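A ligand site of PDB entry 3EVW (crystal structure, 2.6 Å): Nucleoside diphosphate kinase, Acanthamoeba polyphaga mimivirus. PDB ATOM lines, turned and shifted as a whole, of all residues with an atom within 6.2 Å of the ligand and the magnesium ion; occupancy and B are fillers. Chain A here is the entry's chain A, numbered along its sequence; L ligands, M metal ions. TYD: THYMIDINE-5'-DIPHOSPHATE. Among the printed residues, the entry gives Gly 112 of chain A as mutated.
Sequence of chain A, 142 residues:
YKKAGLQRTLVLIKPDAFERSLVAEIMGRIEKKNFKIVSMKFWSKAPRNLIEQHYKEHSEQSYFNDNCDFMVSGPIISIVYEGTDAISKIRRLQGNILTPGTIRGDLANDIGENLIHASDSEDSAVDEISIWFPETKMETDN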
ATOM      1  N   LYS A  14      20.102   7.892   1.870  1.00  0.00           N
ATOM      2  CA  LYS A  14      18.897   7.985   1.031  1.00  0.00           C
ATOM      3  C   LYS A  14      17.962   6.774   1.174  1.00  0.00           C
ATOM      4  O   LYS A  14      18.313   5.761   1.770  1.00  0.00           O
ATOM      5  CB  LYS A  14      19.301   8.195  -0.421  1.00  0.00           C
ATOM      6  CG  LYS A  14      20.206   9.396  -0.627  1.00  0.00           C
ATOM      7  CD  LYS A  14      20.372   9.630  -2.101  1.00  0.00           C
ATOM      8  CE  LYS A  14      21.097  10.926  -2.392  1.00  0.00           C
ATOM      9  NZ  LYS A  14      21.128  11.122  -3.870  1.00  0.00           N
ATOM     10  N   TYR A  55      18.070  20.409  -2.141  1.00  0.00           N
ATOM     11  CA  TYR A  55      18.448  20.309  -3.543  1.00  0.00           C
ATOM     12  C   TYR A  55      18.171  21.570  -4.359  1.00  0.00           C
ATOM     13  O   TYR A  55      18.107  21.530  -5.589  1.00  0.00           O
ATOM     14  CB  TYR A  55      17.750  19.100  -4.172  1.00  0.00           C
ATOM     15  CG  TYR A  55      18.490  17.808  -3.943  1.00  0.00           C
ATOM     16  CD1 TYR A  55      17.896  16.751  -3.266  1.00  0.00           C
ATOM     17  CD2 TYR A  55      19.788  17.634  -4.413  1.00  0.00           C
ATOM     18  CE1 TYR A  55      18.569  15.558  -3.048  1.00  0.00           C
ATOM     19  CE2 TYR A  55      20.469  16.457  -4.210  1.00  0.00           C
ATOM     20  CZ  TYR A  55      19.862  15.417  -3.521  1.00  0.00           C
ATOM     21  OH  TYR A  55      20.557  14.250  -3.320  1.00  0.00           O
ATOM     22  N   HIS A  58      19.448  22.500  -7.737  1.00  0.00           N
ATOM     23  CA  HIS A  58      19.091  21.616  -8.839  1.00  0.00           C
ATOM     24  C   HIS A  58      17.674  21.921  -9.343  1.00  0.00           C
ATOM     25  O   HIS A  58      17.195  21.266 -10.269  1.00  0.00           O
ATOM     26  CB  HIS A  58      19.161  20.137  -8.403  1.00  0.00           C
ATOM     27  CG  HIS A  58      20.507  19.730  -7.873  1.00  0.00           C
ATOM     28  ND1 HIS A  58      21.404  18.994  -8.621  1.00  0.00           N
ATOM     29  CD2 HIS A  58      21.098  19.934  -6.671  1.00  0.00           C
ATOM     30  CE1 HIS A  58      22.501  18.788  -7.912  1.00  0.00           C
ATOM     31  NE2 HIS A  58      22.337  19.352  -6.724  1.00  0.00           N
ATOM     32  N   SER A  62      16.296  18.659 -15.085  1.00  0.00           N
ATOM     33  CA  SER A  62      15.333  17.699 -15.584  1.00  0.00           C
ATOM     34  C   SER A  62      14.997  16.616 -14.557  1.00  0.00           C
ATOM     35  O   SER A  62      13.883  16.073 -14.549  1.00  0.00           O
ATOM     36  CB  SER A  62      15.850  17.051 -16.866  1.00  0.00           C
ATOM     37  OG  SER A  62      17.192  16.648 -16.702  1.00  0.00           O
ATOM     38  N   TYR A  63      15.956  16.307 -13.681  1.00  0.00           N
ATOM     39  CA  TYR A  63      15.768  15.212 -12.727  1.00  0.00           C
ATOM     40  C   TYR A  63      15.149  15.686 -11.420  1.00  0.00           C
ATOM     41  O   TYR A  63      14.776  14.865 -10.580  1.00  0.00           O
ATOM     42  CB  TYR A  63      17.102  14.508 -12.444  1.00  0.00           C
ATOM     43  CG  TYR A  63      18.258  15.418 -12.066  1.00  0.00           C
ATOM     44  CD1 TYR A  63      18.418  15.878 -10.775  1.00  0.00           C
ATOM     45  CD2 TYR A  63      19.190  15.813 -13.027  1.00  0.00           C
ATOM     46  CE1 TYR A  63      19.469  16.718 -10.433  1.00  0.00           C
ATOM     47  CE2 TYR A  63      20.245  16.637 -12.700  1.00  0.00           C
ATOM     48  CZ  TYR A  63      20.390  17.085 -11.407  1.00  0.00           C
ATOM     49  OH  TYR A  63      21.445  17.910 -11.080  1.00  0.00           O
ATOM     50  N   ASP A  66      11.614  13.947 -10.101  1.00  0.00           N
ATOM     51  CA  ASP A  66      11.821  12.509  -9.933  1.00  0.00           C
ATOM     52  C   ASP A  66      12.642  12.265  -8.665  1.00  0.00           C
ATOM     53  O   ASP A  66      12.304  11.407  -7.842  1.00  0.00           O
ATOM     54  CB  ASP A  66      12.557  11.917 -11.144  1.00  0.00           C
ATOM     55  CG  ASP A  66      11.725  11.942 -12.417  1.00  0.00           C
ATOM     56  OD1 ASP A  66      10.486  12.133 -12.327  1.00  0.00           O
ATOM     57  OD2 ASP A  66      12.296  11.760 -13.517  1.00  0.00           O
ATOM     58  N   ASN A  67      13.717  13.032  -8.517  1.00  0.00           N
ATOM     59  CA  ASN A  67      14.607  12.873  -7.386  1.00  0.00           C
ATOM     60  C   ASN A  67      13.948  13.179  -6.046  1.00  0.00           C
ATOM     61  O   ASN A  67      14.158  12.466  -5.066  1.00  0.00           O
ATOM     62  CB  ASN A  67      15.842  13.742  -7.567  1.00  0.00           C
ATOM     63  CG  ASN A  67      16.875  13.486  -6.504  1.00  0.00           C
ATOM     64  OD1 ASN A  67      17.294  14.406  -5.807  1.00  0.00           O
ATOM     65  ND2 ASN A  67      17.271  12.227  -6.353  1.00  0.00           N
ATOM     66  N   ARG A  91      33.097  13.095   0.939  1.00  0.00           N
ATOM     67  CA  ARG A  91      32.676  13.211  -0.451  1.00  0.00           C
ATOM     68  C   ARG A  91      33.349  12.149  -1.312  1.00  0.00           C
ATOM     69  O   ARG A  91      32.730  11.575  -2.185  1.00  0.00           O
ATOM     70  CB  ARG A  91      32.966  14.603  -1.002  1.00  0.00           C
ATOM     71  CG  ARG A  91      31.765  15.261  -1.604  1.00  0.00           C
ATOM     72  CD  ARG A  91      31.504  14.838  -3.033  1.00  0.00           C
ATOM     73  NE  ARG A  91      30.100  14.978  -3.388  1.00  0.00           N
ATOM     74  CZ  ARG A  91      29.649  15.281  -4.606  1.00  0.00           C
ATOM     75  NH1 ARG A  91      30.506  15.521  -5.604  1.00  0.00           N
ATOM     76  NH2 ARG A  91      28.346  15.365  -4.830  1.00  0.00           N
ATOM     77  N   GLN A  94      31.930   8.801  -0.643  1.00  0.00           N
ATOM     78  CA  GLN A  94      30.685   8.629  -1.378  1.00  0.00           C
ATOM     79  C   GLN A  94      30.992   8.195  -2.814  1.00  0.00           C
ATOM     80  O   GLN A  94      30.401   7.253  -3.333  1.00  0.00           O
ATOM     81  CB  GLN A  94      29.885   9.930  -1.402  1.00  0.00           C
ATOM     82  CG  GLN A  94      28.904   9.985  -2.563  1.00  0.00           C
ATOM     83  CD  GLN A  94      28.446  11.393  -2.878  1.00  0.00           C
ATOM     84  OE1 GLN A  94      27.715  12.002  -2.105  1.00  0.00           O
ATOM     85  NE2 GLN A  94      28.866  11.899  -4.013  1.00  0.00           N
ATOM     86  N   GLY A  95      31.923   8.909  -3.434  1.00  0.00           N
ATOM     87  CA  GLY A  95      32.362   8.588  -4.775  1.00  0.00           C
ATOM     88  C   GLY A  95      31.216   8.620  -5.755  1.00  0.00           C
ATOM     89  O   GLY A  95      30.254   9.370  -5.592  1.00  0.00           O
ATOM     90  N   ARG A 104      29.164   4.526  -3.358  1.00  0.00           N
ATOM     91  CA  ARG A 104      28.397   4.387  -4.585  1.00  0.00           C
ATOM     92  C   ARG A 104      29.050   3.403  -5.556  1.00  0.00           C
ATOM     93  O   ARG A 104      28.359   2.584  -6.185  1.00  0.00           O
ATOM     94  CB  ARG A 104      28.191   5.724  -5.253  1.00  0.00           C
ATOM     95  CG  ARG A 104      27.170   6.612  -4.570  1.00  0.00           C
ATOM     96  CD  ARG A 104      27.000   7.869  -5.384  1.00  0.00           C
ATOM     97  NE  ARG A 104      26.132   8.807  -4.708  1.00  0.00           N
ATOM     98  CZ  ARG A 104      26.056  10.100  -4.988  1.00  0.00           C
ATOM     99  NH1 ARG A 104      26.810  10.632  -5.941  1.00  0.00           N
ATOM    100  NH2 ARG A 104      25.233  10.857  -4.279  1.00  0.00           N
ATOM    101  N   ASP A 110      22.624   3.464 -10.095  1.00  0.00           N
ATOM    102  CA  ASP A 110      21.603   4.303 -10.720  1.00  0.00           C
ATOM    103  C   ASP A 110      22.035   5.773 -10.679  1.00  0.00           C
ATOM    104  O   ASP A 110      22.844   6.152  -9.837  1.00  0.00           O
ATOM    105  CB  ASP A 110      20.270   4.117  -9.979  1.00  0.00           C
ATOM    106  CG  ASP A 110      19.079   4.616 -10.776  1.00  0.00           C
ATOM    107  OD1 ASP A 110      18.504   5.659 -10.379  1.00  0.00           O
ATOM    108  OD2 ASP A 110      18.707   3.963 -11.778  1.00  0.00           O
ATOM    109  N   ILE A 111      21.517   6.604 -11.579  1.00  0.00           N
ATOM    110  CA  ILE A 111      21.776   8.035 -11.503  1.00  0.00           C
ATOM    111  C   ILE A 111      21.000   8.664 -10.368  1.00  0.00           C
ATOM    112  O   ILE A 111      21.377   9.721  -9.864  1.00  0.00           O
ATOM    113  CB  ILE A 111      21.388   8.797 -12.777  1.00  0.00           C
ATOM    114  CG1 ILE A 111      20.175   8.143 -13.455  1.00  0.00           C
ATOM    115  CG2 ILE A 111      22.551   8.859 -13.737  1.00  0.00           C
ATOM    116  CD1 ILE A 111      20.542   7.267 -14.671  1.00  0.00           C
ATOM    117  N   GLY A 112      19.908   8.032  -9.989  1.00  0.00           N
ATOM    118  CA  GLY A 112      19.039   8.606  -8.970  1.00  0.00           C
ATOM    119  C   GLY A 112      19.122   7.909  -7.643  1.00  0.00           C
ATOM    120  O   GLY A 112      19.242   8.551  -6.587  1.00  0.00           O
ATOM    121  N   GLU A 113      19.050   6.589  -7.656  1.00  0.00           N
ATOM    122  CA  GLU A 113      19.092   5.827  -6.414  1.00  0.00           C
ATOM    123  C   GLU A 113      20.536   5.441  -6.117  1.00  0.00           C
ATOM    124  O   GLU A 113      21.016   4.385  -6.527  1.00  0.00           O
ATOM    125  CB  GLU A 113      18.183   4.586  -6.508  1.00  0.00           C
ATOM    126  CG  GLU A 113      16.809   4.902  -7.114  1.00  0.00           C
ATOM    127  CD  GLU A 113      15.794   3.764  -6.962  1.00  0.00           C
ATOM    128  OE1 GLU A 113      15.913   2.965  -6.004  1.00  0.00           O
ATOM    129  OE2 GLU A 113      14.867   3.681  -7.799  1.00  0.00           O
ATOM    130  N   ASN A 114      21.223   6.343  -5.419  1.00  0.00           N
ATOM    131  CA  ASN A 114      22.644   6.202  -5.159  1.00  0.00           C
ATOM    132  C   ASN A 114      23.022   6.229  -3.687  1.00  0.00           C
ATOM    133  O   ASN A 114      24.134   6.654  -3.334  1.00  0.00           O
ATOM    134  CB  ASN A 114      23.448   7.261  -5.923  1.00  0.00           C
ATOM    135  CG  ASN A 114      22.890   8.653  -5.729  1.00  0.00           C
ATOM    136  OD1 ASN A 114      22.496   9.052  -4.629  1.00  0.00           O
ATOM    137  ND2 ASN A 114      22.871   9.416  -6.812  1.00  0.00           N
ATOM    138  N   ILE A 116      23.456   7.612  -1.022  1.00  0.00           N
ATOM    139  CA  ILE A 116      24.021   8.609  -0.120  1.00  0.00           C
ATOM    140  C   ILE A 116      24.231   9.979  -0.726  1.00  0.00           C
ATOM    141  O   ILE A 116      24.557  10.123  -1.904  1.00  0.00           O
ATOM    142  CB  ILE A 116      25.386   8.119   0.438  1.00  0.00           C
ATOM    143  CG1 ILE A 116      26.044   9.199   1.305  1.00  0.00           C
ATOM    144  CG2 ILE A 116      26.316   7.653  -0.690  1.00  0.00           C
ATOM    145  CD1 ILE A 116      27.098   8.660   2.233  1.00  0.00           C
ATOM    146  N   HIS A 117      24.067  11.007   0.105  1.00  0.00           N
ATOM    147  CA  HIS A 117      24.483  12.348  -0.268  1.00  0.00           C
ATOM    148  C   HIS A 117      25.543  12.876   0.712  1.00  0.00           C
ATOM    149  O   HIS A 117      25.430  12.716   1.924  1.00  0.00           O
ATOM    150  CB  HIS A 117      23.311  13.327  -0.277  1.00  0.00           C
ATOM    151  CG  HIS A 117      23.733  14.756  -0.173  1.00  0.00           C
ATOM    152  ND1 HIS A 117      23.959  15.543  -1.286  1.00  0.00           N
ATOM    153  CD2 HIS A 117      24.016  15.523   0.905  1.00  0.00           C
ATOM    154  CE1 HIS A 117      24.339  16.752  -0.893  1.00  0.00           C
ATOM    155  NE2 HIS A 117      24.385  16.765   0.423  1.00  0.00           N
ATOM    156  N   ALA A 118      26.554  13.532   0.167  1.00  0.00           N
ATOM    157  CA  ALA A 118      27.539  14.228   0.993  1.00  0.00           C
ATOM    158  C   ALA A 118      27.725  15.666   0.501  1.00  0.00           C
ATOM    159  O   ALA A 118      27.723  15.933  -0.707  1.00  0.00           O
ATOM    160  CB  ALA A 118      28.870  13.451   1.013  1.00  0.00           C
ATOM    161  N   ASP A 120      29.588  18.908  -0.684  1.00  0.00           N
ATOM    162  CA  ASP A 120      30.780  18.964  -1.530  1.00  0.00           C
ATOM    163  C   ASP A 120      31.641  20.202  -1.264  1.00  0.00           C
ATOM    164  O   ASP A 120      32.695  20.351  -1.869  1.00  0.00           O
ATOM    165  CB  ASP A 120      30.410  18.897  -3.010  1.00  0.00           C
ATOM    166  CG  ASP A 120      29.519  20.037  -3.436  1.00  0.00           C
ATOM    167  OD1 ASP A 120      29.248  20.907  -2.566  1.00  0.00           O
ATOM    168  OD2 ASP A 120      29.077  20.075  -4.618  1.00  0.00           O
HETATM  169  PA  TYD L   1      24.496  15.362  -8.594  1.00  0.00           P
HETATM  170  O1A TYD L   1      25.017  16.595  -7.867  1.00  0.00           O
HETATM  171  O2A TYD L   1      24.831  15.131 -10.045  1.00  0.00           O
HETATM  172  O3A TYD L   1      24.922  14.021  -7.770  1.00  0.00           O
HETATM  173  PB  TYD L   1      25.813  14.085  -6.419  1.00  0.00           P
HETATM  174  O1B TYD L   1      24.891  13.569  -5.343  1.00  0.00           O
HETATM  175  O2B TYD L   1      26.156  15.546  -6.216  1.00  0.00           O
HETATM  176  O3B TYD L   1      26.952  13.172  -6.838  1.00  0.00           O
HETATM  177  O5' TYD L   1      22.915  15.223  -8.432  1.00  0.00           O
HETATM  178  C5' TYD L   1      22.333  15.442  -7.154  1.00  0.00           C
HETATM  179  C4' TYD L   1      21.335  14.303  -6.937  1.00  0.00           C
HETATM  180  O4' TYD L   1      20.348  14.344  -7.956  1.00  0.00           O
HETATM  181  C3' TYD L   1      21.959  12.913  -7.078  1.00  0.00           C
HETATM  182  O3' TYD L   1      22.425  12.425  -5.808  1.00  0.00           O
HETATM  183  C2' TYD L   1      20.841  12.042  -7.643  1.00  0.00           C
HETATM  184  C1' TYD L   1      19.928  13.038  -8.340  1.00  0.00           C
HETATM  185  N1  TYD L   1      20.111  12.933  -9.775  1.00  0.00           N
HETATM  186  C2  TYD L   1      19.149  12.223 -10.527  1.00  0.00           C
HETATM  187  O2  TYD L   1      18.168  11.712  -9.946  1.00  0.00           O
HETATM  188  N3  TYD L   1      19.254  12.096 -11.856  1.00  0.00           N
HETATM  189  C4  TYD L   1      20.286  12.636 -12.497  1.00  0.00           C
HETATM  190  O4  TYD L   1      20.391  12.522 -13.741  1.00  0.00           O
HETATM  191  C5  TYD L   1      21.307  13.393 -11.737  1.00  0.00           C
HETATM  192  C5M TYD L   1      22.462  13.991 -12.498  1.00  0.00           C
HETATM  193  C6  TYD L   1      21.170  13.525 -10.353  1.00  0.00           C
HETATM  194 MG    MG M   1      26.393  17.706  -5.989  1.00  0.00          MG
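The guanidinium group (NH2) of Arg 91 lies within salt-bridge range of an oxygen (O3B) of the ligand.
The side-chain amide nitrogen (ND2) of Asn 114 is in hydrogen-bond range of an oxygen (O3') of the ligand (3.2 Å).
NH1 of Arg 104 is in salt-bridge range of O3B of the ligand, at 2.7 Å.
The side-chain amino group of Lys 14 lies within hydrogen-bond range of an oxygen (O3') of the ligand (2.7 Å).
The backbone carbonyl oxygen (O) of Ile 111 sits close to a nitrogen (N1) of the ligand.
Merely in contact with the ligand: Tyr 63 (3.3 Å), His 58 (3.3 Å), Gly 112 (3.4 Å), Asn 67 (3.4 Å), Tyr 55 (3.6 Å) and Gln 94 (3.6 Å).
Hydrophobic or aromatic side chains that line the ligand: Tyr 55, His 58, Tyr 63 and Ile 111.
11 residues have an atom within 4 Å of the ligand: Lys 14, Tyr 55, His 58, Tyr 63, Asn 67, Arg 91, Gln 94, Arg 104, Ile 111, Gly 112 and Asn 114.
Along chain A the residues within 4 Å of the ligand span positions 14 to 114.
The nearest printed residue that does not touch the ligand is His 117 (4.6 Å).
NH2 of Arg 91 touches the magnesium ion (3.3 Å).
OD2 of Asp 120 touches the magnesium ion, 3.8 Å away.
Of the 20 residues printed, 2 come within 4 Å of the magnesium ion.
The nearest printed residue that does not touch the magnesium ion is His 58 (4.4 Å).
The magnesium ion is bound by O2B of the ligand (2.2 Å) and O1A of the ligand (2.6 Å).
NE of Arg 91 lies close to NE2 of Gln 94, 3.4 Å away.
The side-chain hydroxyl of Tyr 63 is in hydrogen-bond range of a ring nitrogen (ND1) of His 58 (2.7 Å).
O of Ile 111 sits at hydrogen-bond distance from ND2 of Asn 114 (3.4 Å).
The backbone NH (N) of Gly 112 lies within hydrogen-bond range of the side-chain carboxylate (OD1) of Asp 110 (2.8 Å).
The backbone NH (N) of Arg 104 sits at hydrogen-bond distance from the backbone carbonyl oxygen (O) of Gln 94.
The side-chain hydroxyl of Tyr 55 is in hydrogen-bond range of the side-chain amino group of Lys 14.
NZ of Lys 14 is in hydrogen-bond range of OD1 of Asn 114 (2.6 Å).
The guanidinium group (NE) of Arg 104 lies within hydrogen-bond range of the backbone carbonyl oxygen (O) of Asn 114, at 3.2 Å.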
